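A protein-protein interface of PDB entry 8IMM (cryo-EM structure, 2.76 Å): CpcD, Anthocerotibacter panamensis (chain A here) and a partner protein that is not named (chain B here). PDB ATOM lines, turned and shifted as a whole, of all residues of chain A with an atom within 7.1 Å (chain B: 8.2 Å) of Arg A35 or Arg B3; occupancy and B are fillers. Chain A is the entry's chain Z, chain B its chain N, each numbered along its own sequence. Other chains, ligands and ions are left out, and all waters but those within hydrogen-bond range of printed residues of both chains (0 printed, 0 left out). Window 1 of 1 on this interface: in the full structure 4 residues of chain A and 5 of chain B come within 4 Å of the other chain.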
ATOM      1  N   ALA A  28       7.150   7.456 -16.980  1.00  0.00           N
ATOM      2  CA  ALA A  28       7.242   8.635 -16.124  1.00  0.00           C
ATOM      3  C   ALA A  28       7.085   9.906 -16.947  1.00  0.00           C
ATOM      4  O   ALA A  28       6.287  10.793 -16.612  1.00  0.00           O
ATOM      5  CB  ALA A  28       8.570   8.637 -15.368  1.00  0.00           C
ATOM      6  N   TYR A  29       7.819   9.990 -18.056  1.00  0.00           N
ATOM      7  CA  TYR A  29       7.598  11.065 -19.012  1.00  0.00           C
ATOM      8  C   TYR A  29       6.187  11.008 -19.569  1.00  0.00           C
ATOM      9  O   TYR A  29       5.547  12.046 -19.774  1.00  0.00           O
ATOM     10  CB  TYR A  29       8.616  10.963 -20.139  1.00  0.00           C
ATOM     11  CG  TYR A  29       8.832  12.233 -20.920  1.00  0.00           C
ATOM     12  CD1 TYR A  29       9.807  13.142 -20.539  1.00  0.00           C
ATOM     13  CD2 TYR A  29       8.078  12.513 -22.050  1.00  0.00           C
ATOM     14  CE1 TYR A  29      10.018  14.301 -21.253  1.00  0.00           C
ATOM     15  CE2 TYR A  29       8.280  13.671 -22.770  1.00  0.00           C
ATOM     16  CZ  TYR A  29       9.255  14.561 -22.367  1.00  0.00           C
ATOM     17  OH  TYR A  29       9.462  15.718 -23.081  1.00  0.00           O
ATOM     18  N   ALA A  30       5.687   9.797 -19.821  1.00  0.00           N
ATOM     19  CA  ALA A  30       4.344   9.652 -20.361  1.00  0.00           C
ATOM     20  C   ALA A  30       3.302  10.210 -19.404  1.00  0.00           C
ATOM     21  O   ALA A  30       2.415  10.960 -19.820  1.00  0.00           O
ATOM     22  CB  ALA A  30       4.053   8.188 -20.679  1.00  0.00           C
ATOM     23  N   THR A  31       3.399   9.877 -18.113  1.00  0.00           N
ATOM     24  CA  THR A  31       2.387  10.364 -17.180  1.00  0.00           C
ATOM     25  C   THR A  31       2.551  11.856 -16.926  1.00  0.00           C
ATOM     26  O   THR A  31       1.560  12.563 -16.710  1.00  0.00           O
ATOM     27  CB  THR A  31       2.423   9.583 -15.861  1.00  0.00           C
ATOM     28  OG1 THR A  31       1.503  10.174 -14.936  1.00  0.00           O
ATOM     29  CG2 THR A  31       3.798   9.613 -15.238  1.00  0.00           C
ATOM     30  N   ASN A  32       3.787  12.363 -16.960  1.00  0.00           N
ATOM     31  CA  ASN A  32       3.971  13.805 -16.838  1.00  0.00           C
ATOM     32  C   ASN A  32       3.315  14.542 -17.999  1.00  0.00           C
ATOM     33  O   ASN A  32       2.647  15.565 -17.801  1.00  0.00           O
ATOM     34  CB  ASN A  32       5.457  14.143 -16.756  1.00  0.00           C
ATOM     35  CG  ASN A  32       6.047  13.840 -15.396  1.00  0.00           C
ATOM     36  OD1 ASN A  32       5.386  13.261 -14.534  1.00  0.00           O
ATOM     37  ND2 ASN A  32       7.299  14.232 -15.192  1.00  0.00           N
ATOM     38  N   LYS A  33       3.485  14.028 -19.219  1.00  0.00           N
ATOM     39  CA  LYS A  33       2.825  14.624 -20.375  1.00  0.00           C
ATOM     40  C   LYS A  33       1.313  14.467 -20.299  1.00  0.00           C
ATOM     41  O   LYS A  33       0.577  15.351 -20.749  1.00  0.00           O
ATOM     42  CB  LYS A  33       3.351  13.998 -21.664  1.00  0.00           C
ATOM     43  CG  LYS A  33       4.559  14.696 -22.260  1.00  0.00           C
ATOM     44  CD  LYS A  33       4.226  16.105 -22.728  1.00  0.00           C
ATOM     45  CE  LYS A  33       5.444  16.768 -23.348  1.00  0.00           C
ATOM     46  NZ  LYS A  33       6.563  16.876 -22.379  1.00  0.00           N
ATOM     47  N   HIS A  34       0.835  13.347 -19.754  1.00  0.00           N
ATOM     48  CA  HIS A  34      -0.600  13.158 -19.573  1.00  0.00           C
ATOM     49  C   HIS A  34      -1.182  14.183 -18.612  1.00  0.00           C
ATOM     50  O   HIS A  34      -2.274  14.708 -18.858  1.00  0.00           O
ATOM     51  CB  HIS A  34      -0.882  11.743 -19.071  1.00  0.00           C
ATOM     52  CG  HIS A  34      -0.546  10.670 -20.060  1.00  0.00           C
ATOM     53  ND1 HIS A  34      -0.128   9.415 -19.678  1.00  0.00           N
ATOM     54  CD2 HIS A  34      -0.581  10.659 -21.412  1.00  0.00           C
ATOM     55  CE1 HIS A  34       0.092   8.678 -20.751  1.00  0.00           C
ATOM     56  NE2 HIS A  34      -0.176   9.410 -21.818  1.00  0.00           N
ATOM     57  N   ARG A  35      -0.486  14.467 -17.508  1.00  0.00           N
ATOM     58  CA  ARG A  35      -0.966  15.492 -16.584  1.00  0.00           C
ATOM     59  C   ARG A  35      -0.917  16.870 -17.222  1.00  0.00           C
ATOM     60  O   ARG A  35      -1.902  17.616 -17.188  1.00  0.00           O
ATOM     61  CB  ARG A  35      -0.147  15.495 -15.295  1.00  0.00           C
ATOM     62  CG  ARG A  35      -0.005  14.177 -14.588  1.00  0.00           C
ATOM     63  CD  ARG A  35       1.132  14.280 -13.595  1.00  0.00           C
ATOM     64  NE  ARG A  35       1.431  13.015 -12.936  1.00  0.00           N
ATOM     65  CZ  ARG A  35       2.543  12.788 -12.247  1.00  0.00           C
ATOM     66  NH1 ARG A  35       3.456  13.742 -12.140  1.00  0.00           N
ATOM     67  NH2 ARG A  35       2.747  11.610 -11.675  1.00  0.00           N
ATOM     68  N   THR A  36       0.231  17.233 -17.798  1.00  0.00           N
ATOM     69  CA  THR A  36       0.395  18.589 -18.302  1.00  0.00           C
ATOM     70  C   THR A  36      -0.312  18.788 -19.637  1.00  0.00           C
ATOM     71  O   THR A  36      -0.729  19.905 -19.959  1.00  0.00           O
ATOM     72  CB  THR A  36       1.881  18.924 -18.418  1.00  0.00           C
ATOM     73  OG1 THR A  36       2.563  18.437 -17.257  1.00  0.00           O
ATOM     74  CG2 THR A  36       2.078  20.428 -18.507  1.00  0.00           C
ATOM     75  N   GLY A  37      -0.457  17.728 -20.421  1.00  0.00           N
ATOM     76  CA  GLY A  37      -1.058  17.830 -21.731  1.00  0.00           C
ATOM     77  C   GLY A  37      -0.018  18.066 -22.811  1.00  0.00           C
ATOM     78  O   GLY A  37       1.047  18.645 -22.578  1.00  0.00           O
ATOM     79  N   TYR A  38      -0.327  17.606 -24.019  1.00  0.00           N
ATOM     80  CA  TYR A  38       0.613  17.729 -25.123  1.00  0.00           C
ATOM     81  C   TYR A  38       0.681  19.177 -25.570  1.00  0.00           C
ATOM     82  O   TYR A  38      -0.335  19.793 -25.907  1.00  0.00           O
ATOM     83  CB  TYR A  38       0.278  16.791 -26.275  1.00  0.00           C
ATOM     84  CG  TYR A  38       1.046  15.513 -26.106  1.00  0.00           C
ATOM     85  CD1 TYR A  38       2.427  15.544 -25.966  1.00  0.00           C
ATOM     86  CD2 TYR A  38       0.407  14.290 -26.042  1.00  0.00           C
ATOM     87  CE1 TYR A  38       3.152  14.397 -25.791  1.00  0.00           C
ATOM     88  CE2 TYR A  38       1.128  13.133 -25.867  1.00  0.00           C
ATOM     89  CZ  TYR A  38       2.499  13.193 -25.741  1.00  0.00           C
ATOM     90  OH  TYR A  38       3.223  12.043 -25.569  1.00  0.00           O
ATOM     91  N   SER B   2       2.696   8.876  -7.929  1.00  0.00           N
ATOM     92  CA  SER B   2       1.848  10.063  -7.931  1.00  0.00           C
ATOM     93  C   SER B   2       2.465  11.169  -7.085  1.00  0.00           C
ATOM     94  O   SER B   2       3.273  10.903  -6.199  1.00  0.00           O
ATOM     95  CB  SER B   2       0.452   9.717  -7.422  1.00  0.00           C
ATOM     96  OG  SER B   2       0.483   9.339  -6.060  1.00  0.00           O
ATOM     97  N   ARG B   3       2.083  12.410  -7.357  1.00  0.00           N
ATOM     98  CA  ARG B   3       2.687  13.561  -6.700  1.00  0.00           C
ATOM     99  C   ARG B   3       1.888  13.887  -5.441  1.00  0.00           C
ATOM    100  O   ARG B   3       0.797  14.456  -5.517  1.00  0.00           O
ATOM    101  CB  ARG B   3       2.743  14.750  -7.652  1.00  0.00           C
ATOM    102  CG  ARG B   3       3.465  14.463  -8.970  1.00  0.00           C
ATOM    103  CD  ARG B   3       4.977  14.328  -8.802  1.00  0.00           C
ATOM    104  NE  ARG B   3       5.377  12.969  -8.439  1.00  0.00           N
ATOM    105  CZ  ARG B   3       5.643  12.004  -9.314  1.00  0.00           C
ATOM    106  NH1 ARG B   3       5.994  10.797  -8.891  1.00  0.00           N
ATOM    107  NH2 ARG B   3       5.576  12.251 -10.614  1.00  0.00           N
ATOM    108  N   THR B   4       2.442  13.527  -4.284  1.00  0.00           N
ATOM    109  CA  THR B   4       1.806  13.698  -2.986  1.00  0.00           C
ATOM    110  C   THR B   4       2.648  14.658  -2.160  1.00  0.00           C
ATOM    111  O   THR B   4       3.593  15.270  -2.663  1.00  0.00           O
ATOM    112  CB  THR B   4       1.649  12.358  -2.263  1.00  0.00           C
ATOM    113  OG1 THR B   4       2.938  11.774  -2.056  1.00  0.00           O
ATOM    114  CG2 THR B   4       0.835  11.417  -3.109  1.00  0.00           C
ATOM    115  N   VAL B   5       2.308  14.789  -0.876  1.00  0.00           N
ATOM    116  CA  VAL B   5       2.947  15.808  -0.047  1.00  0.00           C
ATOM    117  C   VAL B   5       4.431  15.514   0.134  1.00  0.00           C
ATOM    118  O   VAL B   5       5.279  16.371  -0.137  1.00  0.00           O
ATOM    119  CB  VAL B   5       2.229  15.925   1.307  1.00  0.00           C
ATOM    120  CG1 VAL B   5       3.090  16.693   2.291  1.00  0.00           C
ATOM    121  CG2 VAL B   5       0.873  16.587   1.133  1.00  0.00           C
ATOM    122  N   ILE B   6       4.776  14.304   0.572  1.00  0.00           N
ATOM    123  CA  ILE B   6       6.186  13.953   0.714  1.00  0.00           C
ATOM    124  C   ILE B   6       6.876  13.997  -0.641  1.00  0.00           C
ATOM    125  O   ILE B   6       7.995  14.512  -0.775  1.00  0.00           O
ATOM    126  CB  ILE B   6       6.337  12.568   1.366  1.00  0.00           C
ATOM    127  CG1 ILE B   6       5.611  12.509   2.704  1.00  0.00           C
ATOM    128  CG2 ILE B   6       7.800  12.246   1.570  1.00  0.00           C
ATOM    129  CD1 ILE B   6       6.128  13.483   3.718  1.00  0.00           C
ATOM    130  N   THR B   7       6.219  13.457  -1.663  1.00  0.00           N
ATOM    131  CA  THR B   7       6.767  13.466  -3.009  1.00  0.00           C
ATOM    132  C   THR B   7       6.979  14.884  -3.519  1.00  0.00           C
ATOM    133  O   THR B   7       8.003  15.167  -4.143  1.00  0.00           O
ATOM    134  CB  THR B   7       5.840  12.699  -3.946  1.00  0.00           C
ATOM    135  OG1 THR B   7       5.884  11.306  -3.620  1.00  0.00           O
ATOM    136  CG2 THR B   7       6.272  12.879  -5.380  1.00  0.00           C
ATOM    137  N   GLU B   8       6.026  15.785  -3.275  1.00  0.00           N
ATOM    138  CA  GLU B   8       6.194  17.160  -3.734  1.00  0.00           C
ATOM    139  C   GLU B   8       7.344  17.838  -3.012  1.00  0.00           C
ATOM    140  O   GLU B   8       8.089  18.621  -3.609  1.00  0.00           O
ATOM    141  CB  GLU B   8       4.898  17.945  -3.543  1.00  0.00           C
ATOM    142  CG  GLU B   8       3.988  17.895  -4.757  1.00  0.00           C
ATOM    143  CD  GLU B   8       2.521  17.879  -4.393  1.00  0.00           C
ATOM    144  OE1 GLU B   8       1.725  17.317  -5.172  1.00  0.00           O
ATOM    145  OE2 GLU B   8       2.161  18.430  -3.332  1.00  0.00           O
ATOM    146  N   VAL B   9       7.505  17.539  -1.724  1.00  0.00           N
ATOM    147  CA  VAL B   9       8.675  17.994  -0.980  1.00  0.00           C
ATOM    148  C   VAL B   9       9.957  17.558  -1.673  1.00  0.00           C
ATOM    149  O   VAL B   9      10.848  18.371  -1.945  1.00  0.00           O
ATOM    150  CB  VAL B   9       8.613  17.459   0.459  1.00  0.00           C
ATOM    151  CG1 VAL B   9       9.870  17.769   1.176  1.00  0.00           C
ATOM    152  CG2 VAL B   9       7.452  18.089   1.194  1.00  0.00           C
ATOM    153  N   ALA B  11      10.483  16.461  -4.722  1.00  0.00           N
ATOM    154  CA  ALA B  11      10.622  17.001  -6.068  1.00  0.00           C
ATOM    155  C   ALA B  11      11.036  18.467  -6.041  1.00  0.00           C
ATOM    156  O   ALA B  11      11.856  18.898  -6.856  1.00  0.00           O
ATOM    157  CB  ALA B  11       9.315  16.825  -6.839  1.00  0.00           C
ATOM    158  N   ALA B 100      -2.645   8.342   0.594  1.00  0.00           N
ATOM    159  CA  ALA B 100      -1.473   9.080   0.152  1.00  0.00           C
ATOM    160  C   ALA B 100      -1.426  10.498   0.691  1.00  0.00           C
ATOM    161  O   ALA B 100      -0.365  11.127   0.632  1.00  0.00           O
ATOM    162  CB  ALA B 100      -1.431   9.121  -1.374  1.00  0.00           C
ATOM    163  N   SER B 101      -2.542  11.006   1.214  1.00  0.00           N
ATOM    164  CA  SER B 101      -2.653  12.388   1.669  1.00  0.00           C
ATOM    165  C   SER B 101      -2.306  13.365   0.556  1.00  0.00           C
ATOM    166  O   SER B 101      -1.633  14.371   0.784  1.00  0.00           O
ATOM    167  CB  SER B 101      -1.782  12.648   2.897  1.00  0.00           C
ATOM    168  OG  SER B 101      -2.180  11.842   3.990  1.00  0.00           O
ATOM    169  N   GLY B 102      -2.752  13.063  -0.654  1.00  0.00           N
ATOM    170  CA  GLY B 102      -2.545  13.948  -1.782  1.00  0.00           C
ATOM    171  C   GLY B 102      -3.352  13.475  -2.964  1.00  0.00           C
ATOM    172  O   GLY B 102      -3.517  12.273  -3.181  1.00  0.00           O
ATOM    173  N   THR B 103      -3.846  14.428  -3.740  1.00  0.00           N
ATOM    174  CA  THR B 103      -4.691  14.137  -4.887  1.00  0.00           C
ATOM    175  C   THR B 103      -3.936  13.494  -6.039  1.00  0.00           C
ATOM    176  O   THR B 103      -4.492  13.384  -7.132  1.00  0.00           O
ATOM    177  CB  THR B 103      -5.368  15.418  -5.369  1.00  0.00           C
ATOM    178  OG1 THR B 103      -4.369  16.361  -5.774  1.00  0.00           O
ATOM    179  CG2 THR B 103      -6.194  16.029  -4.260  1.00  0.00           C
ATOM    180  N   GLY B 104      -2.694  13.080  -5.827  1.00  0.00           N
ATOM    181  CA  GLY B 104      -1.897  12.487  -6.871  1.00  0.00           C
ATOM    182  C   GLY B 104      -2.526  11.248  -7.471  1.00  0.00           C
ATOM    183  O   GLY B 104      -2.611  11.108  -8.695  1.00  0.00           O
ATOM    184  N   PRO B 105      -2.957  10.307  -6.630  1.00  0.00           N
ATOM    185  CA  PRO B 105      -3.730   9.179  -7.164  1.00  0.00           C
ATOM    186  C   PRO B 105      -4.967   9.615  -7.918  1.00  0.00           C
ATOM    187  O   PRO B 105      -5.224   9.113  -9.018  1.00  0.00           O
ATOM    188  CB  PRO B 105      -4.071   8.381  -5.904  1.00  0.00           C
ATOM    189  CG  PRO B 105      -2.928   8.638  -5.013  1.00  0.00           C
ATOM    190  CD  PRO B 105      -2.520  10.054  -5.245  1.00  0.00           C
ATOM    191  N   LEU B 106      -5.724  10.568  -7.376  1.00  0.00           N
ATOM    192  CA  LEU B 106      -6.900  11.053  -8.085  1.00  0.00           C
ATOM    193  C   LEU B 106      -6.518  11.641  -9.431  1.00  0.00           C
ATOM    194  O   LEU B 106      -7.050  11.229 -10.469  1.00  0.00           O
ATOM    195  CB  LEU B 106      -7.631  12.096  -7.242  1.00  0.00           C
ATOM    196  CG  LEU B 106      -8.801  11.621  -6.387  1.00  0.00           C
ATOM    197  CD1 LEU B 106      -9.182  12.700  -5.399  1.00  0.00           C
ATOM    198  CD2 LEU B 106      -9.984  11.245  -7.257  1.00  0.00           C
ATOM    199  N   ASP B 107      -5.566  12.574  -9.440  1.00  0.00           N
ATOM    200  CA  ASP B 107      -5.175  13.219 -10.685  1.00  0.00           C
ATOM    201  C   ASP B 107      -4.727  12.190 -11.710  1.00  0.00           C
ATOM    202  O   ASP B 107      -5.304  12.091 -12.799  1.00  0.00           O
ATOM    203  CB  ASP B 107      -4.064  14.233 -10.427  1.00  0.00           C
ATOM    204  CG  ASP B 107      -4.462  15.296  -9.426  1.00  0.00           C
ATOM    205  OD1 ASP B 107      -5.601  15.246  -8.921  1.00  0.00           O
ATOM    206  OD2 ASP B 107      -3.630  16.177  -9.134  1.00  0.00           O
ATOM    207  N   ASP B 108      -3.770  11.348 -11.333  1.00  0.00           N
ATOM    208  CA  ASP B 108      -3.132  10.438 -12.269  1.00  0.00           C
ATOM    209  C   ASP B 108      -4.025   9.291 -12.708  1.00  0.00           C
ATOM    210  O   ASP B 108      -3.765   8.706 -13.761  1.00  0.00           O
ATOM    211  CB  ASP B 108      -1.852   9.877 -11.656  1.00  0.00           C
ATOM    212  CG  ASP B 108      -0.776  10.925 -11.510  1.00  0.00           C
ATOM    213  OD1 ASP B 108      -0.756  11.874 -12.318  1.00  0.00           O
ATOM    214  OD2 ASP B 108       0.052  10.804 -10.587  1.00  0.00           O
ATOM    215  N   TYR B 109      -5.065   8.945 -11.949  1.00  0.00           N
ATOM    216  CA  TYR B 109      -5.865   7.795 -12.324  1.00  0.00           C
ATOM    217  C   TYR B 109      -7.249   8.125 -12.854  1.00  0.00           C
ATOM    218  O   TYR B 109      -7.824   7.290 -13.556  1.00  0.00           O
ATOM    219  CB  TYR B 109      -6.003   6.831 -11.143  1.00  0.00           C
ATOM    220  CG  TYR B 109      -4.734   6.078 -10.843  1.00  0.00           C
ATOM    221  CD1 TYR B 109      -4.338   5.016 -11.637  1.00  0.00           C
ATOM    222  CD2 TYR B 109      -3.940   6.419  -9.765  1.00  0.00           C
ATOM    223  CE1 TYR B 109      -3.178   4.327 -11.375  1.00  0.00           C
ATOM    224  CE2 TYR B 109      -2.781   5.729  -9.491  1.00  0.00           C
ATOM    225  CZ  TYR B 109      -2.409   4.681 -10.296  1.00  0.00           C
ATOM    226  OH  TYR B 109      -1.254   3.989 -10.030  1.00  0.00           O
ATOM    227  N   ILE B 111      -8.197  11.956 -13.350  1.00  0.00           N
ATOM    228  CA  ILE B 111      -8.256  13.312 -13.884  1.00  0.00           C
ATOM    229  C   ILE B 111      -7.532  13.398 -15.221  1.00  0.00           C
ATOM    230  O   ILE B 111      -8.081  13.902 -16.205  1.00  0.00           O
ATOM    231  CB  ILE B 111      -7.682  14.312 -12.869  1.00  0.00           C
ATOM    232  CG1 ILE B 111      -8.708  14.609 -11.781  1.00  0.00           C
ATOM    233  CG2 ILE B 111      -7.283  15.605 -13.555  1.00  0.00           C
ATOM    234  CD1 ILE B 111      -8.197  15.533 -10.712  1.00  0.00           C
ATOM    235  N   ALA B 112      -6.301  12.901 -15.283  1.00  0.00           N
ATOM    236  CA  ALA B 112      -5.526  12.958 -16.514  1.00  0.00           C
ATOM    237  C   ALA B 112      -6.182  12.063 -17.554  1.00  0.00           C
ATOM    238  O   ALA B 112      -6.299  10.851 -17.354  1.00  0.00           O
ATOM    239  CB  ALA B 112      -4.083  12.534 -16.265  1.00  0.00           C
ATOM    240  N   GLY B 113      -6.612  12.659 -18.657  1.00  0.00           N
ATOM    241  CA  GLY B 113      -7.299  11.924 -19.691  1.00  0.00           C
ATOM    242  C   GLY B 113      -8.785  11.773 -19.492  1.00  0.00           C
ATOM    243  O   GLY B 113      -9.422  11.053 -20.264  1.00  0.00           O
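The guanidinium group (NH1) of Arg A35 sits close to the guanidinium group (NH2) of Arg B3 (3.0 Å). The side-chain carboxylate (OD1) of Asp B108 is in salt-bridge range of the guanidinium group (NE) of Arg A35, 2.5 Å away.
O of Ala A30 is in hydrogen-bond range of ND1 of His A34, at 3.0 Å. OD1 of Asn A32 sits at hydrogen-bond distance from NH1 of Arg A35 (3.1 Å). N of Ala B112 sits at hydrogen-bond distance from O of Asp B107 (2.8 Å). The guanidinium group of Arg A35 is in hydrogen-bond range of the side-chain hydroxyl of Thr A31 (3.5 Å).
OG1 of Thr A31 touches OD1 of Asp B108 (3.9 Å). Ala B112 touches His A34 (CB to O, 3.8 Å).
Of chain B, only Arg B3 (3.0 Å) and Asp B108 (2.5 Å) come within 4 Å of Arg A35. Of the printed residues of chain A, Arg B3 touches Arg A35. Printed residues of chain B within 4 Å of Thr A31: Asp B108 (3.9 Å). Of the printed residues of chain A, Asp B108 touches Thr A31 and Arg A35. Of the printed residues of chain B, His A34 touches Ala B112. Of the printed residues of chain A, Ala B112 touches His A34. Thr B7 touches none of the printed residues of chain A. The nearest residue of chain B that does not touch Arg A35 is Ser B2 (4.1 Å).
Of the 11 printed residues of chain A, 3 touch a printed residue of chain B. Along chain A the printed residues that touch a printed residue of chain B span positions 31 to 35. Hydrophobic or aromatic side chains of chain B within 4 Å of the printed part of chain A: Ala B112. Among the printed residues, Asp or Glu carboxylates within 4 Å of a Lys or Arg side-chain nitrogen of the other chain: Arg A35 with Asp B108.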
